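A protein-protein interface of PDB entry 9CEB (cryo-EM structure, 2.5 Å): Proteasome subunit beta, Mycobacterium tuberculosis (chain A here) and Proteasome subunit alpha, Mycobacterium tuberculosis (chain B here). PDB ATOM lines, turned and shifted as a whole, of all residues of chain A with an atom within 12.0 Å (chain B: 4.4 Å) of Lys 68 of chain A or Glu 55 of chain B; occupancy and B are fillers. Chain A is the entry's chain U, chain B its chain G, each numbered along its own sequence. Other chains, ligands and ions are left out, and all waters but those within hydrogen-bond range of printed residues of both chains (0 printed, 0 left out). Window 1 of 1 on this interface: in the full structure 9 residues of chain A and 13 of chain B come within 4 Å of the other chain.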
ATOM      1  N   THR A  37     -11.286  28.838   8.911  1.00  0.00           N
ATOM      2  CA  THR A  37     -12.733  28.834   8.740  1.00  0.00           C
ATOM      3  C   THR A  37     -13.473  28.042   9.807  1.00  0.00           C
ATOM      4  O   THR A  37     -14.618  28.374  10.112  1.00  0.00           O
ATOM      5  CB  THR A  37     -13.117  28.297   7.354  1.00  0.00           C
ATOM      6  OG1 THR A  37     -12.331  27.145   7.027  1.00  0.00           O
ATOM      7  CG2 THR A  37     -12.902  29.367   6.300  1.00  0.00           C
ATOM      8  N   ASP A  38     -12.867  27.005  10.373  1.00  0.00           N
ATOM      9  CA  ASP A  38     -13.417  26.346  11.547  1.00  0.00           C
ATOM     10  C   ASP A  38     -12.249  25.755  12.316  1.00  0.00           C
ATOM     11  O   ASP A  38     -11.090  26.057  12.033  1.00  0.00           O
ATOM     12  CB  ASP A  38     -14.495  25.318  11.163  1.00  0.00           C
ATOM     13  CG  ASP A  38     -13.946  24.130  10.391  1.00  0.00           C
ATOM     14  OD1 ASP A  38     -13.463  23.160  11.012  1.00  0.00           O
ATOM     15  OD2 ASP A  38     -13.972  24.183   9.148  1.00  0.00           O
ATOM     16  N   ASP A  39     -12.553  24.905  13.293  1.00  0.00           N
ATOM     17  CA  ASP A  39     -11.520  24.397  14.182  1.00  0.00           C
ATOM     18  C   ASP A  39     -10.515  23.489  13.485  1.00  0.00           C
ATOM     19  O   ASP A  39      -9.438  23.255  14.036  1.00  0.00           O
ATOM     20  CB  ASP A  39     -12.163  23.659  15.349  1.00  0.00           C
ATOM     21  CG  ASP A  39     -12.603  24.589  16.455  1.00  0.00           C
ATOM     22  OD1 ASP A  39     -13.750  25.082  16.410  1.00  0.00           O
ATOM     23  OD2 ASP A  39     -11.796  24.829  17.371  1.00  0.00           O
ATOM     24  N   ARG A  57     -15.630  34.432   5.082  1.00  0.00           N
ATOM     25  CA  ARG A  57     -16.680  34.820   6.018  1.00  0.00           C
ATOM     26  C   ARG A  57     -17.979  34.075   5.744  1.00  0.00           C
ATOM     27  O   ARG A  57     -18.608  33.538   6.663  1.00  0.00           O
ATOM     28  CB  ARG A  57     -16.869  36.335   5.925  1.00  0.00           C
ATOM     29  CG  ARG A  57     -17.609  36.990   7.065  1.00  0.00           C
ATOM     30  CD  ARG A  57     -17.520  38.503   6.945  1.00  0.00           C
ATOM     31  NE  ARG A  57     -18.639  39.211   7.560  1.00  0.00           N
ATOM     32  CZ  ARG A  57     -19.568  39.881   6.893  1.00  0.00           C
ATOM     33  NH1 ARG A  57     -19.533  39.992   5.577  1.00  0.00           N
ATOM     34  NH2 ARG A  57     -20.547  40.471   7.566  1.00  0.00           N
ATOM     35  N   LEU A  58     -18.382  34.014   4.476  1.00  0.00           N
ATOM     36  CA  LEU A  58     -19.591  33.284   4.109  1.00  0.00           C
ATOM     37  C   LEU A  58     -19.473  31.784   4.378  1.00  0.00           C
ATOM     38  O   LEU A  58     -20.417  31.161   4.887  1.00  0.00           O
ATOM     39  CB  LEU A  58     -19.921  33.556   2.648  1.00  0.00           C
ATOM     40  CG  LEU A  58     -21.331  33.190   2.196  1.00  0.00           C
ATOM     41  CD1 LEU A  58     -22.395  33.946   2.976  1.00  0.00           C
ATOM     42  CD2 LEU A  58     -21.476  33.445   0.724  1.00  0.00           C
ATOM     43  N   TYR A  59     -18.325  31.183   4.045  1.00  0.00           N
ATOM     44  CA  TYR A  59     -18.136  29.756   4.295  1.00  0.00           C
ATOM     45  C   TYR A  59     -18.134  29.426   5.784  1.00  0.00           C
ATOM     46  O   TYR A  59     -18.723  28.419   6.207  1.00  0.00           O
ATOM     47  CB  TYR A  59     -16.855  29.284   3.607  1.00  0.00           C
ATOM     48  CG  TYR A  59     -16.633  27.795   3.641  1.00  0.00           C
ATOM     49  CD1 TYR A  59     -17.534  26.923   3.053  1.00  0.00           C
ATOM     50  CD2 TYR A  59     -15.487  27.268   4.219  1.00  0.00           C
ATOM     51  CE1 TYR A  59     -17.329  25.572   3.082  1.00  0.00           C
ATOM     52  CE2 TYR A  59     -15.267  25.925   4.242  1.00  0.00           C
ATOM     53  CZ  TYR A  59     -16.191  25.079   3.671  1.00  0.00           C
ATOM     54  OH  TYR A  59     -15.976  23.730   3.693  1.00  0.00           O
ATOM     55  N   ALA A  60     -17.489  30.264   6.598  1.00  0.00           N
ATOM     56  CA  ALA A  60     -17.500  30.051   8.039  1.00  0.00           C
ATOM     57  C   ALA A  60     -18.900  30.210   8.622  1.00  0.00           C
ATOM     58  O   ALA A  60     -19.284  29.465   9.536  1.00  0.00           O
ATOM     59  CB  ALA A  60     -16.517  31.004   8.707  1.00  0.00           C
ATOM     60  N   VAL A  61     -19.677  31.171   8.113  1.00  0.00           N
ATOM     61  CA  VAL A  61     -21.049  31.341   8.591  1.00  0.00           C
ATOM     62  C   VAL A  61     -21.878  30.104   8.276  1.00  0.00           C
ATOM     63  O   VAL A  61     -22.632  29.620   9.125  1.00  0.00           O
ATOM     64  CB  VAL A  61     -21.673  32.626   8.008  1.00  0.00           C
ATOM     65  CG1 VAL A  61     -23.163  32.671   8.231  1.00  0.00           C
ATOM     66  CG2 VAL A  61     -21.049  33.840   8.654  1.00  0.00           C
ATOM     67  N   GLU A  62     -21.730  29.561   7.066  1.00  0.00           N
ATOM     68  CA  GLU A  62     -22.482  28.367   6.685  1.00  0.00           C
ATOM     69  C   GLU A  62     -22.137  27.173   7.574  1.00  0.00           C
ATOM     70  O   GLU A  62     -23.029  26.439   8.033  1.00  0.00           O
ATOM     71  CB  GLU A  62     -22.212  28.041   5.223  1.00  0.00           C
ATOM     72  CG  GLU A  62     -23.024  26.883   4.711  1.00  0.00           C
ATOM     73  CD  GLU A  62     -22.817  26.610   3.243  1.00  0.00           C
ATOM     74  OE1 GLU A  62     -21.737  26.947   2.720  1.00  0.00           O
ATOM     75  OE2 GLU A  62     -23.752  26.083   2.607  1.00  0.00           O
ATOM     76  N   LEU A  63     -20.841  26.966   7.834  1.00  0.00           N
ATOM     77  CA  LEU A  63     -20.416  25.830   8.650  1.00  0.00           C
ATOM     78  C   LEU A  63     -20.922  25.943  10.089  1.00  0.00           C
ATOM     79  O   LEU A  63     -21.398  24.962  10.678  1.00  0.00           O
ATOM     80  CB  LEU A  63     -18.894  25.721   8.628  1.00  0.00           C
ATOM     81  CG  LEU A  63     -18.234  25.173   7.361  1.00  0.00           C
ATOM     82  CD1 LEU A  63     -16.764  24.946   7.601  1.00  0.00           C
ATOM     83  CD2 LEU A  63     -18.892  23.905   6.861  1.00  0.00           C
ATOM     84  N   GLU A  64     -20.823  27.141  10.674  1.00  0.00           N
ATOM     85  CA  GLU A  64     -21.288  27.313  12.047  1.00  0.00           C
ATOM     86  C   GLU A  64     -22.807  27.260  12.147  1.00  0.00           C
ATOM     87  O   GLU A  64     -23.341  26.798  13.159  1.00  0.00           O
ATOM     88  CB  GLU A  64     -20.762  28.622  12.622  1.00  0.00           C
ATOM     89  CG  GLU A  64     -20.320  28.516  14.062  1.00  0.00           C
ATOM     90  CD  GLU A  64     -20.250  29.858  14.752  1.00  0.00           C
ATOM     91  OE1 GLU A  64     -21.318  30.425  15.051  1.00  0.00           O
ATOM     92  OE2 GLU A  64     -19.127  30.343  15.003  1.00  0.00           O
ATOM     93  N   HIS A  65     -23.511  27.725  11.114  1.00  0.00           N
ATOM     94  CA  HIS A  65     -24.965  27.653  11.101  1.00  0.00           C
ATOM     95  C   HIS A  65     -25.436  26.207  11.108  1.00  0.00           C
ATOM     96  O   HIS A  65     -26.354  25.850  11.859  1.00  0.00           O
ATOM     97  CB  HIS A  65     -25.482  28.406   9.874  1.00  0.00           C
ATOM     98  CG  HIS A  65     -26.971  28.499   9.783  1.00  0.00           C
ATOM     99  ND1 HIS A  65     -27.720  29.292  10.620  1.00  0.00           N
ATOM    100  CD2 HIS A  65     -27.849  27.921   8.931  1.00  0.00           C
ATOM    101  CE1 HIS A  65     -28.996  29.190  10.299  1.00  0.00           C
ATOM    102  NE2 HIS A  65     -29.101  28.363   9.277  1.00  0.00           N
ATOM    103  N   TYR A  66     -24.803  25.353  10.294  1.00  0.00           N
ATOM    104  CA  TYR A  66     -25.140  23.933  10.338  1.00  0.00           C
ATOM    105  C   TYR A  66     -24.836  23.336  11.704  1.00  0.00           C
ATOM    106  O   TYR A  66     -25.645  22.574  12.252  1.00  0.00           O
ATOM    107  CB  TYR A  66     -24.382  23.161   9.261  1.00  0.00           C
ATOM    108  CG  TYR A  66     -24.767  21.702   9.217  1.00  0.00           C
ATOM    109  CD1 TYR A  66     -24.165  20.773  10.057  1.00  0.00           C
ATOM    110  CD2 TYR A  66     -25.744  21.257   8.345  1.00  0.00           C
ATOM    111  CE1 TYR A  66     -24.528  19.462  10.035  1.00  0.00           C
ATOM    112  CE2 TYR A  66     -26.108  19.943   8.306  1.00  0.00           C
ATOM    113  CZ  TYR A  66     -25.497  19.048   9.151  1.00  0.00           C
ATOM    114  OH  TYR A  66     -25.860  17.729   9.113  1.00  0.00           O
ATOM    115  N   GLU A  67     -23.666  23.656  12.259  1.00  0.00           N
ATOM    116  CA  GLU A  67     -23.293  23.092  13.551  1.00  0.00           C
ATOM    117  C   GLU A  67     -24.284  23.480  14.645  1.00  0.00           C
ATOM    118  O   GLU A  67     -24.565  22.685  15.547  1.00  0.00           O
ATOM    119  CB  GLU A  67     -21.881  23.544  13.906  1.00  0.00           C
ATOM    120  CG  GLU A  67     -21.078  22.539  14.658  1.00  0.00           C
ATOM    121  CD  GLU A  67     -21.325  22.601  16.139  1.00  0.00           C
ATOM    122  OE1 GLU A  67     -21.621  23.701  16.648  1.00  0.00           O
ATOM    123  OE2 GLU A  67     -21.223  21.547  16.798  1.00  0.00           O
ATOM    124  N   LYS A  68     -24.821  24.704  14.583  1.00  0.00           N
ATOM    125  CA  LYS A  68     -25.772  25.157  15.596  1.00  0.00           C
ATOM    126  C   LYS A  68     -27.153  24.541  15.396  1.00  0.00           C
ATOM    127  O   LYS A  68     -27.822  24.191  16.372  1.00  0.00           O
ATOM    128  CB  LYS A  68     -25.857  26.680  15.579  1.00  0.00           C
ATOM    129  CG  LYS A  68     -24.987  27.381  16.610  1.00  0.00           C
ATOM    130  CD  LYS A  68     -25.275  28.861  16.644  1.00  0.00           C
ATOM    131  CE  LYS A  68     -25.001  29.505  15.302  1.00  0.00           C
ATOM    132  NZ  LYS A  68     -25.286  30.957  15.343  1.00  0.00           N
ATOM    133  N   LEU A  69     -27.599  24.404  14.141  1.00  0.00           N
ATOM    134  CA  LEU A  69     -28.899  23.786  13.888  1.00  0.00           C
ATOM    135  C   LEU A  69     -28.912  22.310  14.253  1.00  0.00           C
ATOM    136  O   LEU A  69     -29.851  21.837  14.896  1.00  0.00           O
ATOM    137  CB  LEU A  69     -29.301  23.944  12.427  1.00  0.00           C
ATOM    138  CG  LEU A  69     -29.682  25.331  11.925  1.00  0.00           C
ATOM    139  CD1 LEU A  69     -29.774  25.332  10.415  1.00  0.00           C
ATOM    140  CD2 LEU A  69     -30.984  25.783  12.552  1.00  0.00           C
ATOM    141  N   GLU A  70     -27.897  21.556  13.833  1.00  0.00           N
ATOM    142  CA  GLU A  70     -27.951  20.105  13.937  1.00  0.00           C
ATOM    143  C   GLU A  70     -27.315  19.554  15.202  1.00  0.00           C
ATOM    144  O   GLU A  70     -27.540  18.387  15.521  1.00  0.00           O
ATOM    145  CB  GLU A  70     -27.289  19.452  12.718  1.00  0.00           C
ATOM    146  CG  GLU A  70     -28.008  19.636  11.382  1.00  0.00           C
ATOM    147  CD  GLU A  70     -29.528  19.722  11.471  1.00  0.00           C
ATOM    148  OE1 GLU A  70     -30.159  18.929  12.207  1.00  0.00           O
ATOM    149  OE2 GLU A  70     -30.101  20.578  10.770  1.00  0.00           O
ATOM    150  N   GLY A  71     -26.524  20.344  15.922  1.00  0.00           N
ATOM    151  CA  GLY A  71     -25.868  19.871  17.116  1.00  0.00           C
ATOM    152  C   GLY A  71     -24.535  19.194  16.895  1.00  0.00           C
ATOM    153  O   GLY A  71     -23.801  18.983  17.866  1.00  0.00           O
ATOM    154  N   VAL A  72     -24.191  18.854  15.656  1.00  0.00           N
ATOM    155  CA  VAL A  72     -22.901  18.234  15.351  1.00  0.00           C
ATOM    156  C   VAL A  72     -22.298  18.914  14.138  1.00  0.00           C
ATOM    157  O   VAL A  72     -23.010  19.458  13.285  1.00  0.00           O
ATOM    158  CB  VAL A  72     -23.033  16.714  15.085  1.00  0.00           C
ATOM    159  CG1 VAL A  72     -23.308  15.971  16.375  1.00  0.00           C
ATOM    160  CG2 VAL A  72     -24.122  16.433  14.067  1.00  0.00           C
ATOM    161  N   PRO A  73     -20.971  18.917  14.050  1.00  0.00           N
ATOM    162  CA  PRO A  73     -20.322  19.438  12.842  1.00  0.00           C
ATOM    163  C   PRO A  73     -20.490  18.508  11.652  1.00  0.00           C
ATOM    164  O   PRO A  73     -20.731  17.308  11.791  1.00  0.00           O
ATOM    165  CB  PRO A  73     -18.851  19.559  13.250  1.00  0.00           C
ATOM    166  CG  PRO A  73     -18.691  18.629  14.386  1.00  0.00           C
ATOM    167  CD  PRO A  73     -19.996  18.632  15.115  1.00  0.00           C
ATOM    168  N   LEU A  74     -20.367  19.088  10.465  1.00  0.00           N
ATOM    169  CA  LEU A  74     -20.420  18.317   9.238  1.00  0.00           C
ATOM    170  C   LEU A  74     -19.188  17.422   9.123  1.00  0.00           C
ATOM    171  O   LEU A  74     -18.134  17.695   9.702  1.00  0.00           O
ATOM    172  CB  LEU A  74     -20.485  19.243   8.029  1.00  0.00           C
ATOM    173  CG  LEU A  74     -21.834  19.765   7.537  1.00  0.00           C
ATOM    174  CD1 LEU A  74     -21.615  20.952   6.629  1.00  0.00           C
ATOM    175  CD2 LEU A  74     -22.647  18.707   6.832  1.00  0.00           C
ATOM    176  N   THR A  75     -19.328  16.339   8.361  1.00  0.00           N
ATOM    177  CA  THR A  75     -18.173  15.540   7.976  1.00  0.00           C
ATOM    178  C   THR A  75     -17.342  16.284   6.931  1.00  0.00           C
ATOM    179  O   THR A  75     -17.782  17.269   6.337  1.00  0.00           O
ATOM    180  CB  THR A  75     -18.612  14.174   7.439  1.00  0.00           C
ATOM    181  OG1 THR A  75     -19.314  14.332   6.199  1.00  0.00           O
ATOM    182  CG2 THR A  75     -19.510  13.462   8.428  1.00  0.00           C
ATOM    183  N   LYS A  79     -18.450  19.213   4.103  1.00  0.00           N
ATOM    184  CA  LYS A  79     -17.788  20.500   3.916  1.00  0.00           C
ATOM    185  C   LYS A  79     -17.308  20.691   2.485  1.00  0.00           C
ATOM    186  O   LYS A  79     -17.455  21.782   1.917  1.00  0.00           O
ATOM    187  CB  LYS A  79     -16.624  20.625   4.887  1.00  0.00           C
ATOM    188  CG  LYS A  79     -17.001  20.467   6.319  1.00  0.00           C
ATOM    189  CD  LYS A  79     -15.812  20.604   7.211  1.00  0.00           C
ATOM    190  CE  LYS A  79     -16.196  20.363   8.639  1.00  0.00           C
ATOM    191  NZ  LYS A  79     -15.043  19.902   9.438  1.00  0.00           N
ATOM    192  N   SER B  54     -30.170  25.529  24.475  1.00  0.00           N
ATOM    193  CA  SER B  54     -29.376  25.645  23.260  1.00  0.00           C
ATOM    194  C   SER B  54     -28.728  27.019  23.215  1.00  0.00           C
ATOM    195  O   SER B  54     -29.082  27.922  23.971  1.00  0.00           O
ATOM    196  CB  SER B  54     -30.240  25.410  22.016  1.00  0.00           C
ATOM    197  OG  SER B  54     -29.514  25.581  20.811  1.00  0.00           O
ATOM    198  N   GLU B  55     -27.767  27.171  22.319  1.00  0.00           N
ATOM    199  CA  GLU B  55     -27.187  28.475  22.044  1.00  0.00           C
ATOM    200  C   GLU B  55     -27.816  29.107  20.805  1.00  0.00           C
ATOM    201  O   GLU B  55     -28.305  28.414  19.913  1.00  0.00           O
ATOM    202  CB  GLU B  55     -25.678  28.358  21.871  1.00  0.00           C
ATOM    203  CG  GLU B  55     -25.245  28.177  20.446  1.00  0.00           C
ATOM    204  CD  GLU B  55     -23.782  28.438  20.239  1.00  0.00           C
ATOM    205  OE1 GLU B  55     -22.971  27.546  20.551  1.00  0.00           O
ATOM    206  OE2 GLU B  55     -23.443  29.531  19.752  1.00  0.00           O
ATOM    207  N   LEU B  56     -27.814  30.440  20.769  1.00  0.00           N
ATOM    208  CA  LEU B  56     -28.290  31.195  19.615  1.00  0.00           C
ATOM    209  C   LEU B  56     -27.177  31.913  18.869  1.00  0.00           C
ATOM    210  O   LEU B  56     -27.087  31.801  17.649  1.00  0.00           O
ATOM    211  CB  LEU B  56     -29.364  32.207  20.035  1.00  0.00           C
ATOM    212  CG  LEU B  56     -30.645  31.611  20.611  1.00  0.00           C
ATOM    213  CD1 LEU B  56     -31.480  32.665  21.317  1.00  0.00           C
ATOM    214  CD2 LEU B  56     -31.441  30.915  19.505  1.00  0.00           C
ATOM    215  N   TYR B  57     -26.333  32.655  19.574  1.00  0.00           N
ATOM    216  CA  TYR B  57     -25.204  33.365  18.985  1.00  0.00           C
ATOM    217  C   TYR B  57     -24.030  33.232  19.946  1.00  0.00           C
ATOM    218  O   TYR B  57     -24.046  32.398  20.855  1.00  0.00           O
ATOM    219  CB  TYR B  57     -25.571  34.822  18.672  1.00  0.00           C
ATOM    220  CG  TYR B  57     -24.927  35.342  17.415  1.00  0.00           C
ATOM    221  CD1 TYR B  57     -25.117  34.706  16.203  1.00  0.00           C
ATOM    222  CD2 TYR B  57     -24.097  36.454  17.452  1.00  0.00           C
ATOM    223  CE1 TYR B  57     -24.517  35.169  15.063  1.00  0.00           C
ATOM    224  CE2 TYR B  57     -23.494  36.923  16.321  1.00  0.00           C
ATOM    225  CZ  TYR B  57     -23.710  36.276  15.126  1.00  0.00           C
ATOM    226  OH  TYR B  57     -23.111  36.742  13.990  1.00  0.00           O
ATOM    227  N   VAL B  60     -25.317  34.661  23.417  1.00  0.00           N
ATOM    228  CA  VAL B  60     -26.754  34.602  23.664  1.00  0.00           C
ATOM    229  C   VAL B  60     -27.165  33.145  23.832  1.00  0.00           C
ATOM    230  O   VAL B  60     -26.763  32.286  23.039  1.00  0.00           O
ATOM    231  CB  VAL B  60     -27.556  35.267  22.528  1.00  0.00           C
ATOM    232  CG1 VAL B  60     -29.021  35.409  22.920  1.00  0.00           C
ATOM    233  CG2 VAL B  60     -26.973  36.623  22.182  1.00  0.00           C
ATOM    234  N   ARG B  75     -36.619  27.940  18.173  1.00  0.00           N
ATOM    235  CA  ARG B  75     -35.167  27.994  18.306  1.00  0.00           C
ATOM    236  C   ARG B  75     -34.477  28.018  16.947  1.00  0.00           C
ATOM    237  O   ARG B  75     -33.513  28.769  16.746  1.00  0.00           O
ATOM    238  CB  ARG B  75     -34.698  26.808  19.141  1.00  0.00           C
ATOM    239  CG  ARG B  75     -33.205  26.628  19.184  1.00  0.00           C
ATOM    240  CD  ARG B  75     -32.820  25.241  19.655  1.00  0.00           C
ATOM    241  NE  ARG B  75     -32.943  24.254  18.589  1.00  0.00           N
ATOM    242  CZ  ARG B  75     -31.926  23.765  17.893  1.00  0.00           C
ATOM    243  NH1 ARG B  75     -30.682  24.125  18.134  1.00  0.00           N
ATOM    244  NH2 ARG B  75     -32.166  22.900  16.918  1.00  0.00           N
ATOM    245  N   ILE B  79     -32.129  31.122  15.537  1.00  0.00           N
ATOM    246  CA  ILE B  79     -30.775  30.922  15.022  1.00  0.00           C
ATOM    247  C   ILE B  79     -30.647  31.518  13.623  1.00  0.00           C
ATOM    248  O   ILE B  79     -29.651  32.180  13.305  1.00  0.00           O
ATOM    249  CB  ILE B  79     -30.413  29.425  15.047  1.00  0.00           C
ATOM    250  CG1 ILE B  79     -30.095  28.971  16.468  1.00  0.00           C
ATOM    251  CG2 ILE B  79     -29.232  29.107  14.145  1.00  0.00           C
ATOM    252  CD1 ILE B  79     -29.996  27.486  16.604  1.00  0.00           C
ATOM    253  N   ASP B  83     -28.105  34.646  12.718  1.00  0.00           N
ATOM    254  CA  ASP B  83     -27.052  34.460  11.721  1.00  0.00           C
ATOM    255  C   ASP B  83     -27.168  35.465  10.583  1.00  0.00           C
ATOM    256  O   ASP B  83     -26.160  36.023  10.129  1.00  0.00           O
ATOM    257  CB  ASP B  83     -27.083  33.038  11.170  1.00  0.00           C
ATOM    258  CG  ASP B  83     -26.272  32.074  11.991  1.00  0.00           C
ATOM    259  OD1 ASP B  83     -25.292  32.514  12.605  1.00  0.00           O
ATOM    260  OD2 ASP B  83     -26.605  30.873  12.006  1.00  0.00           O
ATOM    261  N   ARG B 220     -17.149  32.162  21.859  1.00  0.00           N
ATOM    262  CA  ARG B 220     -18.368  31.401  22.088  1.00  0.00           C
ATOM    263  C   ARG B 220     -18.469  31.049  23.563  1.00  0.00           C
ATOM    264  O   ARG B 220     -17.616  30.335  24.090  1.00  0.00           O
ATOM    265  CB  ARG B 220     -18.382  30.133  21.242  1.00  0.00           C
ATOM    266  CG  ARG B 220     -18.409  30.393  19.762  1.00  0.00           C
ATOM    267  CD  ARG B 220     -19.394  29.488  19.073  1.00  0.00           C
ATOM    268  NE  ARG B 220     -18.747  28.552  18.167  1.00  0.00           N
ATOM    269  CZ  ARG B 220     -19.287  27.413  17.758  1.00  0.00           C
ATOM    270  NH1 ARG B 220     -20.489  27.035  18.160  1.00  0.00           N
ATOM    271  NH2 ARG B 220     -18.610  26.639  16.915  1.00  0.00           N
ATOM    272  N   PHE B 222     -21.059  29.444  25.154  1.00  0.00           N
ATOM    273  CA  PHE B 222     -21.938  28.326  25.481  1.00  0.00           C
ATOM    274  C   PHE B 222     -21.152  27.021  25.547  1.00  0.00           C
ATOM    275  O   PHE B 222     -20.353  26.726  24.654  1.00  0.00           O
ATOM    276  CB  PHE B 222     -23.056  28.211  24.442  1.00  0.00           C
ATOM    277  CG  PHE B 222     -24.101  27.192  24.783  1.00  0.00           C
ATOM    278  CD1 PHE B 222     -25.138  27.503  25.641  1.00  0.00           C
ATOM    279  CD2 PHE B 222     -24.042  25.914  24.250  1.00  0.00           C
ATOM    280  CE1 PHE B 222     -26.093  26.567  25.956  1.00  0.00           C
ATOM    281  CE2 PHE B 222     -24.993  24.975  24.565  1.00  0.00           C
ATOM    282  CZ  PHE B 222     -26.020  25.301  25.417  1.00  0.00           C
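Lys 68 of chain A touches six residues of chain B.
Of chain A, only Lys 68 comes within 4 Å of Leu 56 of chain B.
Of chain A, only Lys 68 comes within 4 Å of Tyr 57 of chain B.
Printed residues of chain A within 4 Å of Ile 79 of chain B: His 65 (3.8 Å) and Lys 68 (3.95 Å).
Arg 220 of chain B touches two residues of chain A.
Printed residues of chain B within 4 Å of Glu 64 of chain A: Arg 220 (3.7 Å).
Of the printed residues of chain B, Glu 67 of chain A touches Arg 220 (3.8 Å).
Of the printed residues of chain A, Arg 75 of chain B touches Lys 68 and Leu 69.
Lys 79 of chain A touches none of the printed residues of chain B.
The nearest printed residue of chain B that does not touch Lys 68 of chain A is Arg 220 of chain B (4.8 Å).
The nearest printed residue of chain B that does not touch Glu 67 of chain A is Glu 55 of chain B (5.6 Å).
The side-chain amino group of Lys 68 of chain A sits at hydrogen-bond distance from the backbone carbonyl oxygen of Leu 56 of chain B (3.0 Å).
The guanidinium group of Arg 75 of chain B is in hydrogen-bond range of the backbone carbonyl oxygen of Leu 69 of chain A (3.3 Å).
OD1 of Asp 83 of chain B is in salt-bridge range of NZ of Lys 68 of chain A (3.1 Å).
NH1 of Arg 75 of chain B sits at hydrogen-bond distance from O of Lys 68 of chain A, at 3.4 Å.
NE of Arg 220 of chain B is in salt-bridge range of OE2 of Glu 64 of chain A, at 3.7 Å.
NH1 of Arg 220 of chain B is in salt-bridge range of OE1 of Glu 67 of chain A (3.8 Å).
A ring nitrogen (ND1) of His 65 of chain A sits close to the side-chain carboxylate (OD2) of Asp 83 of chain B (2.4 Å).
Printed residues of chain A that touch a printed residue of chain B: Glu 64, His 65, Glu 67, Lys 68 and Leu 69.
Hydrophobic or aromatic side chains of chain A that line the printed part of chain B: His 65.
Hydrophobic or aromatic side chains of chain B that line the printed part of chain A: Tyr 57 and Ile 79.
His 65 of chain A touches Ile 79 of chain B (ND1 to CG2, 3.8 Å).
Glu 55 of chain B touches Lys 68 of chain A (OE2 to CD, 3.7 Å).
CD1 of Tyr 57 of chain B touches NZ of Lys 68 of chain A, 3.9 Å away.
O of Lys 68 of chain A touches CD1 of Ile 79 of chain B, 3.95 Å away.
OE1 of Glu 55 of chain B lies within salt-bridge range of NH1 of Arg 220 of chain B (3.5 Å).
The guanidinium group (NH1) of Arg 75 of chain B is in hydrogen-bond range of the side-chain hydroxyl (OG) of Ser 54 of chain B (3.3 Å).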
